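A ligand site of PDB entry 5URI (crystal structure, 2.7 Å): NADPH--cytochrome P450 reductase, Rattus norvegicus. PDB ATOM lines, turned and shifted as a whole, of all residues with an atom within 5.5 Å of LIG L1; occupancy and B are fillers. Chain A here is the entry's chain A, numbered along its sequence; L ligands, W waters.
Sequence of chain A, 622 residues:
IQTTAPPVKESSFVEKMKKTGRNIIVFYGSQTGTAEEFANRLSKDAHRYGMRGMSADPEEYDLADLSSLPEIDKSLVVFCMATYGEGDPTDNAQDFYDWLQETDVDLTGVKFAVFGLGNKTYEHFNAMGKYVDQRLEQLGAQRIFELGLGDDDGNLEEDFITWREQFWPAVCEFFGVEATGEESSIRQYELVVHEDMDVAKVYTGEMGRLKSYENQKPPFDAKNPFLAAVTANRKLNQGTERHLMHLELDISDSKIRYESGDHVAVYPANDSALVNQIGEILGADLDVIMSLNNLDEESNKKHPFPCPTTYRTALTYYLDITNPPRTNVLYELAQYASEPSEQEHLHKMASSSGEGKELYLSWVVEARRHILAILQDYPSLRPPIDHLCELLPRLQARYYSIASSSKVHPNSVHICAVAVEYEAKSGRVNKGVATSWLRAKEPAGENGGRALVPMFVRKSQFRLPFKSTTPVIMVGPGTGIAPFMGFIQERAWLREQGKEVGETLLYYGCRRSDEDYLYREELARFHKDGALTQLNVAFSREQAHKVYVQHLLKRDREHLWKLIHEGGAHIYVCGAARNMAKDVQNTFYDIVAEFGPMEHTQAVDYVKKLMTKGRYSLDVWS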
ATOM      1  N   HIS A 263     -26.279  18.354  -2.459  1.00  0.00           N
ATOM      2  CA  HIS A 263     -25.946  16.944  -2.447  1.00  0.00           C
ATOM      3  C   HIS A 263     -26.072  16.365  -3.838  1.00  0.00           C
ATOM      4  O   HIS A 263     -26.860  16.849  -4.656  1.00  0.00           O
ATOM      5  CB  HIS A 263     -26.868  16.195  -1.490  1.00  0.00           C
ATOM      6  CG  HIS A 263     -26.725  16.626  -0.059  1.00  0.00           C
ATOM      7  ND1 HIS A 263     -27.728  17.257   0.640  1.00  0.00           N
ATOM      8  CD2 HIS A 263     -25.681  16.512   0.801  1.00  0.00           C
ATOM      9  CE1 HIS A 263     -27.318  17.511   1.865  1.00  0.00           C
ATOM     10  NE2 HIS A 263     -26.079  17.069   1.997  1.00  0.00           N
ATOM     11  N   THR A 322     -27.471  -6.274   0.162  1.00  0.00           N
ATOM     12  CA  THR A 322     -26.458  -6.154   1.220  1.00  0.00           C
ATOM     13  C   THR A 322     -26.924  -5.726   2.616  1.00  0.00           C
ATOM     14  O   THR A 322     -26.198  -5.899   3.586  1.00  0.00           O
ATOM     15  CB  THR A 322     -25.366  -5.156   0.822  1.00  0.00           C
ATOM     16  OG1 THR A 322     -25.915  -3.830   0.854  1.00  0.00           O
ATOM     17  CG2 THR A 322     -24.847  -5.430  -0.583  1.00  0.00           C
ATOM     18  N   ASN A 323     -28.104  -5.133   2.744  1.00  0.00           N
ATOM     19  CA  ASN A 323     -28.538  -4.725   4.070  1.00  0.00           C
ATOM     20  C   ASN A 323     -29.293  -5.820   4.780  1.00  0.00           C
ATOM     21  O   ASN A 323     -30.065  -6.553   4.171  1.00  0.00           O
ATOM     22  CB  ASN A 323     -29.390  -3.472   4.009  1.00  0.00           C
ATOM     23  CG  ASN A 323     -28.581  -2.241   3.701  1.00  0.00           C
ATOM     24  OD1 ASN A 323     -27.433  -2.129   4.141  1.00  0.00           O
ATOM     25  ND2 ASN A 323     -29.154  -1.309   2.956  1.00  0.00           N
ATOM     26  N   ARG A 368     -24.755  -8.146  10.729  1.00  0.00           N
ATOM     27  CA  ARG A 368     -24.761  -7.551   9.404  1.00  0.00           C
ATOM     28  C   ARG A 368     -24.777  -8.636   8.327  1.00  0.00           C
ATOM     29  O   ARG A 368     -24.025  -8.581   7.346  1.00  0.00           O
ATOM     30  CB  ARG A 368     -23.558  -6.620   9.223  1.00  0.00           C
ATOM     31  CG  ARG A 368     -23.604  -5.376  10.096  1.00  0.00           C
ATOM     32  CD  ARG A 368     -24.804  -4.486   9.749  1.00  0.00           C
ATOM     33  NE  ARG A 368     -24.736  -3.999   8.365  1.00  0.00           N
ATOM     34  CZ  ARG A 368     -25.609  -3.142   7.825  1.00  0.00           C
ATOM     35  NH1 ARG A 368     -25.453  -2.765   6.561  1.00  0.00           N
ATOM     36  NH2 ARG A 368     -26.624  -2.661   8.535  1.00  0.00           N
ATOM     37  N   ARG A 398     -27.269   6.711  -3.235  1.00  0.00           N
ATOM     38  CA  ARG A 398     -26.473   7.150  -2.087  1.00  0.00           C
ATOM     39  C   ARG A 398     -26.151   8.630  -2.305  1.00  0.00           C
ATOM     40  O   ARG A 398     -25.768   9.028  -3.399  1.00  0.00           O
ATOM     41  CB  ARG A 398     -25.171   6.351  -1.993  1.00  0.00           C
ATOM     42  CG  ARG A 398     -25.219   5.056  -1.197  1.00  0.00           C
ATOM     43  CD  ARG A 398     -26.149   4.032  -1.783  1.00  0.00           C
ATOM     44  NE  ARG A 398     -25.986   2.738  -1.143  1.00  0.00           N
ATOM     45  CZ  ARG A 398     -26.832   1.722  -1.288  1.00  0.00           C
ATOM     46  NH1 ARG A 398     -26.594   0.573  -0.663  1.00  0.00           N
ATOM     47  NH2 ARG A 398     -27.916   1.856  -2.043  1.00  0.00           N
ATOM     48  N   TYR A 399     -26.321   9.450  -1.263  1.00  0.00           N
ATOM     49  CA  TYR A 399     -26.029  10.882  -1.353  1.00  0.00           C
ATOM     50  C   TYR A 399     -24.600  11.234  -0.924  1.00  0.00           C
ATOM     51  O   TYR A 399     -23.998  10.557  -0.093  1.00  0.00           O
ATOM     52  CB  TYR A 399     -27.009  11.710  -0.502  1.00  0.00           C
ATOM     53  CG  TYR A 399     -28.413  11.657  -1.038  1.00  0.00           C
ATOM     54  CD1 TYR A 399     -29.237  10.554  -0.797  1.00  0.00           C
ATOM     55  CD2 TYR A 399     -28.890  12.663  -1.880  1.00  0.00           C
ATOM     56  CE1 TYR A 399     -30.480  10.450  -1.396  1.00  0.00           C
ATOM     57  CE2 TYR A 399     -30.133  12.570  -2.479  1.00  0.00           C
ATOM     58  CZ  TYR A 399     -30.920  11.459  -2.244  1.00  0.00           C
ATOM     59  OH  TYR A 399     -32.139  11.336  -2.878  1.00  0.00           O
ATOM     60  N   TYR A 400     -24.076  12.317  -1.500  1.00  0.00           N
ATOM     61  CA  TYR A 400     -22.737  12.800  -1.190  1.00  0.00           C
ATOM     62  C   TYR A 400     -22.765  14.331  -1.251  1.00  0.00           C
ATOM     63  O   TYR A 400     -23.402  14.914  -2.123  1.00  0.00           O
ATOM     64  CB  TYR A 400     -21.748  12.219  -2.195  1.00  0.00           C
ATOM     65  CG  TYR A 400     -21.573  10.743  -2.003  1.00  0.00           C
ATOM     66  CD1 TYR A 400     -20.720  10.258  -1.013  1.00  0.00           C
ATOM     67  CD2 TYR A 400     -22.307   9.828  -2.741  1.00  0.00           C
ATOM     68  CE1 TYR A 400     -20.632   8.888  -0.748  1.00  0.00           C
ATOM     69  CE2 TYR A 400     -22.233   8.457  -2.477  1.00  0.00           C
ATOM     70  CZ  TYR A 400     -21.389   8.002  -1.481  1.00  0.00           C
ATOM     71  OH  TYR A 400     -21.332   6.661  -1.189  1.00  0.00           O
ATOM     72  N   SER A 401     -22.083  14.986  -0.317  1.00  0.00           N
ATOM     73  CA  SER A 401     -22.044  16.433  -0.296  1.00  0.00           C
ATOM     74  C   SER A 401     -21.062  16.883  -1.364  1.00  0.00           C
ATOM     75  O   SER A 401     -19.891  16.535  -1.301  1.00  0.00           O
ATOM     76  CB  SER A 401     -21.571  16.946   1.066  1.00  0.00           C
ATOM     77  OG  SER A 401     -22.333  16.401   2.129  1.00  0.00           O
ATOM     78  N   CYS A 416     -16.243  13.524  -2.230  1.00  0.00           N
ATOM     79  CA  CYS A 416     -15.217  13.202  -1.253  1.00  0.00           C
ATOM     80  C   CYS A 416     -15.791  12.093  -0.395  1.00  0.00           C
ATOM     81  O   CYS A 416     -16.705  12.322   0.396  1.00  0.00           O
ATOM     82  CB  CYS A 416     -14.913  14.430  -0.403  1.00  0.00           C
ATOM     83  SG  CYS A 416     -13.822  14.113   0.980  1.00  0.00           S
ATOM     84  N   ALA A 417     -15.269  10.882  -0.523  1.00  0.00           N
ATOM     85  CA  ALA A 417     -15.818   9.772   0.244  1.00  0.00           C
ATOM     86  C   ALA A 417     -14.817   8.732   0.709  1.00  0.00           C
ATOM     87  O   ALA A 417     -13.773   8.506   0.071  1.00  0.00           O
ATOM     88  CB  ALA A 417     -16.907   9.092  -0.569  1.00  0.00           C
ATOM     89  N   VAL A 418     -15.147   8.078   1.818  1.00  0.00           N
ATOM     90  CA  VAL A 418     -14.325   7.017   2.369  1.00  0.00           C
ATOM     91  C   VAL A 418     -14.993   5.688   2.033  1.00  0.00           C
ATOM     92  O   VAL A 418     -16.130   5.430   2.447  1.00  0.00           O
ATOM     93  CB  VAL A 418     -14.150   7.143   3.922  1.00  0.00           C
ATOM     94  CG1 VAL A 418     -15.506   7.249   4.616  1.00  0.00           C
ATOM     95  CG2 VAL A 418     -13.381   5.948   4.439  1.00  0.00           C
ATOM     96  N   VAL A 420     -16.395   2.103   2.112  1.00  0.00           N
ATOM     97  CA  VAL A 420     -16.805   1.263   3.231  1.00  0.00           C
ATOM     98  C   VAL A 420     -16.438  -0.202   2.984  1.00  0.00           C
ATOM     99  O   VAL A 420     -16.796  -0.797   1.961  1.00  0.00           O
ATOM    100  CB  VAL A 420     -18.312   1.377   3.530  1.00  0.00           C
ATOM    101  CG1 VAL A 420     -18.693   0.419   4.646  1.00  0.00           C
ATOM    102  CG2 VAL A 420     -18.660   2.799   3.942  1.00  0.00           C
ATOM    103  N   TYR A 422     -15.627  -3.494   5.878  1.00  0.00           N
ATOM    104  CA  TYR A 422     -15.376  -3.869   7.269  1.00  0.00           C
ATOM    105  C   TYR A 422     -15.579  -5.340   7.526  1.00  0.00           C
ATOM    106  O   TYR A 422     -16.089  -6.062   6.671  1.00  0.00           O
ATOM    107  CB  TYR A 422     -16.285  -3.074   8.194  1.00  0.00           C
ATOM    108  CG  TYR A 422     -17.745  -3.264   7.901  1.00  0.00           C
ATOM    109  CD1 TYR A 422     -18.375  -2.514   6.897  1.00  0.00           C
ATOM    110  CD2 TYR A 422     -18.511  -4.190   8.606  1.00  0.00           C
ATOM    111  CE1 TYR A 422     -19.729  -2.696   6.615  1.00  0.00           C
ATOM    112  CE2 TYR A 422     -19.865  -4.373   8.323  1.00  0.00           C
ATOM    113  CZ  TYR A 422     -20.467  -3.620   7.335  1.00  0.00           C
ATOM    114  OH  TYR A 422     -21.808  -3.791   7.067  1.00  0.00           O
ATOM    115  N   GLU A 423     -15.168  -5.770   8.705  1.00  0.00           N
ATOM    116  CA  GLU A 423     -15.325  -7.163   9.117  1.00  0.00           C
ATOM    117  C   GLU A 423     -16.601  -7.239   9.932  1.00  0.00           C
ATOM    118  O   GLU A 423     -16.715  -6.626  10.995  1.00  0.00           O
ATOM    119  CB  GLU A 423     -14.143  -7.619   9.977  1.00  0.00           C
ATOM    120  CG  GLU A 423     -13.225  -6.469  10.439  1.00  0.00           C
ATOM    121  CD  GLU A 423     -12.453  -6.750  11.732  1.00  0.00           C
ATOM    122  OE1 GLU A 423     -13.039  -6.589  12.826  1.00  0.00           O
ATOM    123  OE2 GLU A 423     -11.260  -7.140  11.642  1.00  0.00           O
ATOM    124  N   LYS A 431     -18.766  -5.084   2.045  1.00  0.00           N
ATOM    125  CA  LYS A 431     -18.295  -3.950   1.268  1.00  0.00           C
ATOM    126  C   LYS A 431     -19.444  -3.006   0.949  1.00  0.00           C
ATOM    127  O   LYS A 431     -20.520  -3.433   0.527  1.00  0.00           O
ATOM    128  CB  LYS A 431     -17.611  -4.410  -0.028  1.00  0.00           C
ATOM    129  CG  LYS A 431     -16.211  -5.029   0.150  1.00  0.00           C
ATOM    130  CD  LYS A 431     -15.319  -4.831  -1.084  1.00  0.00           C
ATOM    131  CE  LYS A 431     -14.865  -3.369  -1.219  1.00  0.00           C
ATOM    132  NZ  LYS A 431     -13.998  -3.042  -2.415  1.00  0.00           N
ATOM    133  N   GLY A 432     -19.215  -1.711   1.150  1.00  0.00           N
ATOM    134  CA  GLY A 432     -20.221  -0.696   0.856  1.00  0.00           C
ATOM    135  C   GLY A 432     -20.549  -0.690  -0.620  1.00  0.00           C
ATOM    136  O   GLY A 432     -19.665  -0.652  -1.476  1.00  0.00           O
ATOM    137  N   VAL A 433     -21.836  -0.708  -0.926  1.00  0.00           N
ATOM    138  CA  VAL A 433     -22.278  -0.727  -2.307  1.00  0.00           C
ATOM    139  C   VAL A 433     -21.790   0.405  -3.211  1.00  0.00           C
ATOM    140  O   VAL A 433     -21.081   0.156  -4.178  1.00  0.00           O
ATOM    141  CB  VAL A 433     -23.812  -0.776  -2.380  1.00  0.00           C
ATOM    142  CG1 VAL A 433     -24.272  -0.809  -3.853  1.00  0.00           C
ATOM    143  CG2 VAL A 433     -24.312  -1.983  -1.623  1.00  0.00           C
ATOM    144  N   ALA A 434     -22.177   1.630  -2.895  1.00  0.00           N
ATOM    145  CA  ALA A 434     -21.798   2.776  -3.725  1.00  0.00           C
ATOM    146  C   ALA A 434     -20.310   3.100  -3.745  1.00  0.00           C
ATOM    147  O   ALA A 434     -19.757   3.480  -4.791  1.00  0.00           O
ATOM    148  CB  ALA A 434     -22.596   4.017  -3.274  1.00  0.00           C
ATOM    149  N   THR A 435     -19.664   2.957  -2.594  1.00  0.00           N
ATOM    150  CA  THR A 435     -18.247   3.248  -2.503  1.00  0.00           C
ATOM    151  C   THR A 435     -17.351   2.238  -3.232  1.00  0.00           C
ATOM    152  O   THR A 435     -16.435   2.643  -3.933  1.00  0.00           O
ATOM    153  CB  THR A 435     -17.832   3.409  -1.028  1.00  0.00           C
ATOM    154  OG1 THR A 435     -18.318   2.303  -0.266  1.00  0.00           O
ATOM    155  CG2 THR A 435     -18.403   4.718  -0.480  1.00  0.00           C
ATOM    156  N   SER A 436     -17.611   0.939  -3.102  1.00  0.00           N
ATOM    157  CA  SER A 436     -16.781  -0.046  -3.812  1.00  0.00           C
ATOM    158  C   SER A 436     -16.950   0.232  -5.312  1.00  0.00           C
ATOM    159  O   SER A 436     -15.975   0.147  -6.104  1.00  0.00           O
ATOM    160  CB  SER A 436     -17.249  -1.475  -3.544  1.00  0.00           C
ATOM    161  OG  SER A 436     -17.374  -1.746  -2.168  1.00  0.00           O
ATOM    162  N   THR A 479     -14.366  13.158   6.882  1.00  0.00           N
ATOM    163  CA  THR A 479     -14.917  13.443   5.560  1.00  0.00           C
ATOM    164  C   THR A 479     -15.880  14.620   5.568  1.00  0.00           C
ATOM    165  O   THR A 479     -16.350  15.029   4.515  1.00  0.00           O
ATOM    166  CB  THR A 479     -15.641  12.213   4.951  1.00  0.00           C
ATOM    167  OG1 THR A 479     -16.630  11.739   5.878  1.00  0.00           O
ATOM    168  CG2 THR A 479     -14.652  11.100   4.667  1.00  0.00           C
ATOM    169  N   ALA A 482     -15.919  17.770   3.214  1.00  0.00           N
ATOM    170  CA  ALA A 482     -16.453  17.725   1.852  1.00  0.00           C
ATOM    171  C   ALA A 482     -17.113  18.988   1.308  1.00  0.00           C
ATOM    172  O   ALA A 482     -16.613  19.577   0.348  1.00  0.00           O
ATOM    173  CB  ALA A 482     -17.453  16.569   1.741  1.00  0.00           C
ATOM    174  N   ASP A 619     -25.247  19.208   8.617  1.00  0.00           N
ATOM    175  CA  ASP A 619     -25.245  18.294   7.508  1.00  0.00           C
ATOM    176  C   ASP A 619     -24.528  17.054   7.982  1.00  0.00           C
ATOM    177  O   ASP A 619     -23.384  16.802   7.596  1.00  0.00           O
ATOM    178  CB  ASP A 619     -24.540  18.901   6.299  1.00  0.00           C
ATOM    179  CG  ASP A 619     -24.716  18.062   5.048  1.00  0.00           C
ATOM    180  OD1 ASP A 619     -25.873  17.712   4.748  1.00  0.00           O
ATOM    181  OD2 ASP A 619     -23.715  17.752   4.375  1.00  0.00           O
ATOM    182  N   VAL A 620     -25.194  16.331   8.876  1.00  0.00           N
ATOM    183  CA  VAL A 620     -24.656  15.090   9.422  1.00  0.00           C
ATOM    184  C   VAL A 620     -25.405  13.937   8.789  1.00  0.00           C
ATOM    185  O   VAL A 620     -26.572  14.056   8.427  1.00  0.00           O
ATOM    186  CB  VAL A 620     -24.814  15.011  10.947  1.00  0.00           C
ATOM    187  CG1 VAL A 620     -23.991  16.110  11.613  1.00  0.00           C
ATOM    188  CG2 VAL A 620     -26.283  15.140  11.332  1.00  0.00           C
ATOM    189  N   TRP A 621     -24.719  12.818   8.650  1.00  0.00           N
ATOM    190  CA  TRP A 621     -25.334  11.655   8.043  1.00  0.00           C
ATOM    191  C   TRP A 621     -25.062  10.371   8.800  1.00  0.00           C
ATOM    192  O   TRP A 621     -24.095  10.280   9.579  1.00  0.00           O
ATOM    193  CB  TRP A 621     -24.874  11.546   6.596  1.00  0.00           C
ATOM    194  CG  TRP A 621     -23.372  11.564   6.386  1.00  0.00           C
ATOM    195  CD1 TRP A 621     -22.498  10.528   6.598  1.00  0.00           C
ATOM    196  CD2 TRP A 621     -22.586  12.637   5.840  1.00  0.00           C
ATOM    197  NE1 TRP A 621     -21.227  10.887   6.215  1.00  0.00           N
ATOM    198  CE2 TRP A 621     -21.252  12.165   5.736  1.00  0.00           C
ATOM    199  CE3 TRP A 621     -22.884  13.938   5.422  1.00  0.00           C
ATOM    200  CZ2 TRP A 621     -20.213  12.965   5.227  1.00  0.00           C
ATOM    201  CZ3 TRP A 621     -21.852  14.718   4.921  1.00  0.00           C
ATOM    202  CH2 TRP A 621     -20.531  14.226   4.830  1.00  0.00           C
ATOM    203  N   SER A 622     -25.928   9.382   8.576  1.00  0.00           N
ATOM    204  CA  SER A 622     -25.841   8.061   9.193  1.00  0.00           C
ATOM    205  C   SER A 622     -25.416   8.092  10.658  1.00  0.00           C
ATOM    206  O   SER A 622     -25.449   9.180  11.287  1.00  0.00           O
ATOM    207  CB  SER A 622     -24.886   7.163   8.386  1.00  0.00           C
ATOM    208  OG  SER A 622     -23.568   7.685   8.368  1.00  0.00           O
ATOM    209  OXT SER A 622     -25.058   6.998  11.180  1.00  0.00           O
HETATM  210  P1  LIG L   1     -23.576   0.831   2.131  1.00  0.00           P
HETATM  211  O1  LIG L   1     -23.775  -0.427   1.378  1.00  0.00           O
HETATM  212  O2  LIG L   1     -24.619   1.870   2.076  1.00  0.00           O
HETATM  213  O3  LIG L   1     -23.309   0.462   3.671  1.00  0.00           O
HETATM  214  C1  LIG L   1     -23.498   1.469   4.673  1.00  0.00           C
HETATM  215  C2  LIG L   1     -23.797   0.764   6.004  1.00  0.00           C
HETATM  216  O4  LIG L   1     -22.681  -0.050   6.382  1.00  0.00           O
HETATM  217  C3  LIG L   1     -23.869   1.773   7.129  1.00  0.00           C
HETATM  218  O5  LIG L   1     -25.167   2.384   7.104  1.00  0.00           O
HETATM  219  C4  LIG L   1     -23.790   0.808   8.296  1.00  0.00           C
HETATM  220  O6  LIG L   1     -25.086   0.265   8.570  1.00  0.00           O
HETATM  221  C5  LIG L   1     -22.852  -0.284   7.783  1.00  0.00           C
HETATM  222  N1  LIG L   1     -21.496  -0.173   8.372  1.00  0.00           N
HETATM  223  C6  LIG L   1     -20.451   0.791   7.966  1.00  0.00           C
HETATM  224  N2  LIG L   1     -19.336   0.361   8.829  1.00  0.00           N
HETATM  225  C7  LIG L   1     -19.758  -0.639   9.604  1.00  0.00           C
HETATM  226  C8  LIG L   1     -19.081  -1.318  10.530  1.00  0.00           C
HETATM  227  N3  LIG L   1     -17.760  -1.146  10.528  1.00  0.00           N
HETATM  228  N4  LIG L   1     -19.655  -2.270  11.278  1.00  0.00           N
HETATM  229  C9  LIG L   1     -21.003  -2.570  11.069  1.00  0.00           C
HETATM  230  N5  LIG L   1     -21.682  -1.843  10.086  1.00  0.00           N
HETATM  231  C10 LIG L   1     -21.045  -0.895   9.390  1.00  0.00           C
HETATM  232  N6  LIG L   1     -20.385   9.925   2.723  1.00  0.00           N
HETATM  233  C11 LIG L   1     -19.135  10.391   2.294  1.00  0.00           C
HETATM  234  O7  LIG L   1     -18.133   9.693   2.438  1.00  0.00           O
HETATM  235  N7  LIG L   1     -19.013  11.700   1.812  1.00  0.00           N
HETATM  236  C12 LIG L   1     -20.133  12.532   1.752  1.00  0.00           C
HETATM  237  O8  LIG L   1     -20.015  13.672   1.316  1.00  0.00           O
HETATM  238  C13 LIG L   1     -21.370  12.067   2.181  1.00  0.00           C
HETATM  239  N8  LIG L   1     -22.411  12.910   2.265  1.00  0.00           N
HETATM  240  C14 LIG L   1     -23.598  12.457   2.675  1.00  0.00           C
HETATM  241  C15 LIG L   1     -24.689  13.325   2.721  1.00  0.00           C
HETATM  242  C16 LIG L   1     -25.938  12.858   3.108  1.00  0.00           C
HETATM  243  C17 LIG L   1     -27.016  13.737   3.154  1.00  0.00           C
HETATM  244  C18 LIG L   1     -26.110  11.522   3.447  1.00  0.00           C
HETATM  245  C19 LIG L   1     -27.370  11.032   3.778  1.00  0.00           C
HETATM  246  C20 LIG L   1     -25.019  10.654   3.401  1.00  0.00           C
HETATM  247  C21 LIG L   1     -23.769  11.111   3.001  1.00  0.00           C
HETATM  248  N9  LIG L   1     -22.715  10.280   2.931  1.00  0.00           N
HETATM  249  C22 LIG L   1     -21.500  10.768   2.670  1.00  0.00           C
HETATM  250  C23 LIG L   1     -22.865   8.835   3.260  1.00  0.00           C
HETATM  251  C24 LIG L   1     -23.279   8.039   2.020  1.00  0.00           C
HETATM  252  O9  LIG L   1     -24.585   8.448   1.611  1.00  0.00           O
HETATM  253  C25 LIG L   1     -23.281   6.532   2.300  1.00  0.00           C
HETATM  254  O10 LIG L   1     -23.942   6.280   3.543  1.00  0.00           O
HETATM  255  C26 LIG L   1     -21.843   6.013   2.377  1.00  0.00           C
HETATM  256  O11 LIG L   1     -21.113   6.453   1.230  1.00  0.00           O
HETATM  257  C27 LIG L   1     -21.843   4.480   2.437  1.00  0.00           C
HETATM  258  O12 LIG L   1     -22.586   3.957   1.342  1.00  0.00           O
HETATM  259  P2  LIG L   1     -22.133   2.623   0.564  1.00  0.00           P
HETATM  260  O13 LIG L   1     -20.718   2.779   0.120  1.00  0.00           O
HETATM  261  O14 LIG L   1     -23.162   2.292  -0.447  1.00  0.00           O
HETATM  262  O15 LIG L   1     -22.175   1.478   1.696  1.00  0.00           O
HETATM  263  N1  LG2 L   2     -35.006  11.956  11.694  1.00  0.00           N
HETATM  264  C1  LG2 L   2     -35.611  12.800  12.550  1.00  0.00           C
HETATM  265  O1  LG2 L   2     -36.279  12.379  13.501  1.00  0.00           O
HETATM  266  N2  LG2 L   2     -35.451  14.149  12.316  1.00  0.00           N
HETATM  267  C2  LG2 L   2     -34.715  14.753  11.285  1.00  0.00           C
HETATM  268  O2  LG2 L   2     -34.716  15.976  11.282  1.00  0.00           O
HETATM  269  C3  LG2 L   2     -34.063  13.880  10.375  1.00  0.00           C
HETATM  270  N3  LG2 L   2     -33.318  14.454   9.324  1.00  0.00           N
HETATM  271  C4  LG2 L   2     -32.699  13.521   8.478  1.00  0.00           C
HETATM  272  C5  LG2 L   2     -31.909  14.077   7.401  1.00  0.00           C
HETATM  273  C6  LG2 L   2     -31.232  13.246   6.476  1.00  0.00           C
HETATM  274  C7  LG2 L   2     -30.432  13.983   5.373  1.00  0.00           C
HETATM  275  C8  LG2 L   2     -31.307  11.750   6.589  1.00  0.00           C
HETATM  276  C9  LG2 L   2     -30.699  10.846   5.763  1.00  0.00           C
HETATM  277  C10 LG2 L   2     -32.061  11.204   7.618  1.00  0.00           C
HETATM  278  C11 LG2 L   2     -32.777  12.054   8.590  1.00  0.00           C
HETATM  279  N4  LG2 L   2     -33.593  11.538   9.715  1.00  0.00           N
HETATM  280  C12 LG2 L   2     -34.264  12.479  10.637  1.00  0.00           C
HETATM  281  C13 LG2 L   2     -33.739  10.099   9.902  1.00  0.00           C
HETATM  282  C14 LG2 L   2     -34.902   9.483   9.071  1.00  0.00           C
HETATM  283  O3  LG2 L   2     -36.167  10.129   9.492  1.00  0.00           O
HETATM  284  C15 LG2 L   2     -34.989   7.989   9.305  1.00  0.00           C
HETATM  285  O4  LG2 L   2     -33.722   7.433   8.860  1.00  0.00           O
HETATM  286  C16 LG2 L   2     -36.183   7.411   8.472  1.00  0.00           C
HETATM  287  O5  LG2 L   2     -36.125   6.002   8.849  1.00  0.00           O
HETATM  288  C17 LG2 L   2     -35.973   7.434   6.971  1.00  0.00           C
HETATM  289  O6  LG2 L   2     -37.132   6.912   6.236  1.00  0.00           O
HETATM  290  P1  LG2 L   2     -37.254   6.759   4.665  1.00  0.00           P
HETATM  291  O7  LG2 L   2     -36.293   5.720   4.194  1.00  0.00           O
HETATM  292  O8  LG2 L   2     -37.156   8.225   4.121  1.00  0.00           O
HETATM  293  O9  LG2 L   2     -38.740   6.170   4.530  1.00  0.00           O
HETATM  294  O   HOH W   1     -26.396   7.724   4.986  1.00  0.00           O
HETATM  295  O   HOH W   2     -27.197   8.054   1.206  1.00  0.00           O
HETATM  296  O   HOH W   3     -18.558  14.017  -1.063  1.00  0.00           O
HETATM  297  O   HOH W   4     -22.822  -2.250   4.812  1.00  0.00           O
HETATM  298  O   HOH W   5     -22.614  -3.003   2.468  1.00  0.00           O
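The side-chain hydroxyl of Thr 435 is in hydrogen-bond range of an oxygen (O13) of LIG L1 (2.5 Å). An oxygen (O7) of LIG L1 sits at hydrogen-bond distance from the backbone NH of Val 418, 3.5 Å away. NH2 of Arg 368 is in hydrogen-bond range of O6 of LIG L1 (3.3 Å). An oxygen (O1) of LIG L1 lies within hydrogen-bond range of the backbone NH (N) of Val 433. The side-chain hydroxyl (OG) of Ser 401 sits at hydrogen-bond distance from a nitrogen (N8) of LIG L1 (3.5 Å). N of Thr 435 is in hydrogen-bond range of O13 of LIG L1. O14 of LIG L1 lies within hydrogen-bond range of N of Ala 434, 2.7 Å away. N of Ser 401 lies within hydrogen-bond range of O8 of LIG L1 (2.9 Å). An oxygen (O9) of LIG L1 sits at hydrogen-bond distance from the backbone carbonyl oxygen (O) of Tyr 399, at 2.8 Å. OH of Tyr 400 lies within hydrogen-bond range of O11 of LIG L1, at 2.4 Å. O of Cys 416 is in hydrogen-bond range of N7 of LIG L1 (2.8 Å). An oxygen (O14) of LIG L1 lies within salt-bridge range of the guanidinium group (NE) of Arg 398, 2.9 Å away.
NE of Arg 368 lies within hydrogen-bond range of OH of Tyr 422 (3.2 Å). N of Val 420 is in hydrogen-bond range of OG1 of Thr 435 (3.1 Å). The guanidinium group (NH1) of Arg 368 sits at hydrogen-bond distance from the side-chain amide oxygen (OD1) of Asn 323 (3.2 Å). O of Gly 432 is in hydrogen-bond range of OG of Ser 436. The side-chain hydroxyl (OG1) of Thr 435 lies within hydrogen-bond range of the backbone carbonyl oxygen (O) of Gly 432 (3.5 Å). The backbone carbonyl oxygen (O) of Val 420 sits at hydrogen-bond distance from the backbone NH (N) of Gly 432. The side-chain carboxylate (OD2) of Asp 619 lies within hydrogen-bond range of the side-chain hydroxyl (OG) of Ser 401 (3.0 Å). OD1 of Asp 619 sits at hydrogen-bond distance from NE2 of His 263 (2.8 Å).
Merely in contact with LIG L1: His 263, Ala 417, Val 420, Tyr 422, Gly 432, Ala 482 and Trp 621. Hydrophobic or aromatic side chains that line LIG L1: His 263, Tyr 399, Tyr 400, Ala 417, Val 420, Tyr 422, Val 433, Ala 434, Ala 482 and Trp 621. 17 residues have an atom within 4 Å of LIG L1: His 263, Arg 368, Arg 398, Tyr 399, Tyr 400, Ser 401, Cys 416, Ala 417, Val 418, Val 420, Tyr 422, Gly 432, Val 433, Ala 434, Thr 435, Ala 482 and Trp 621.
Water W2 lies within hydrogen-bond range of an oxygen (O9) of LIG L1 (2.7 Å) and the backbone NH of Tyr 399 (3.0 Å). Water W4 lies within hydrogen-bond range of an oxygen (O4) of LIG L1, the side-chain hydroxyl (OH) of Tyr 422 and the guanidinium group (NH1) of Arg 368. Water W3 lies within hydrogen-bond range of N of Cys 416, O8 of LIG L1 and O of Ser 401. Water W5 bridges O of Lys 431 (2.9 Å) and O1 of LIG L1 (3.0 Å).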
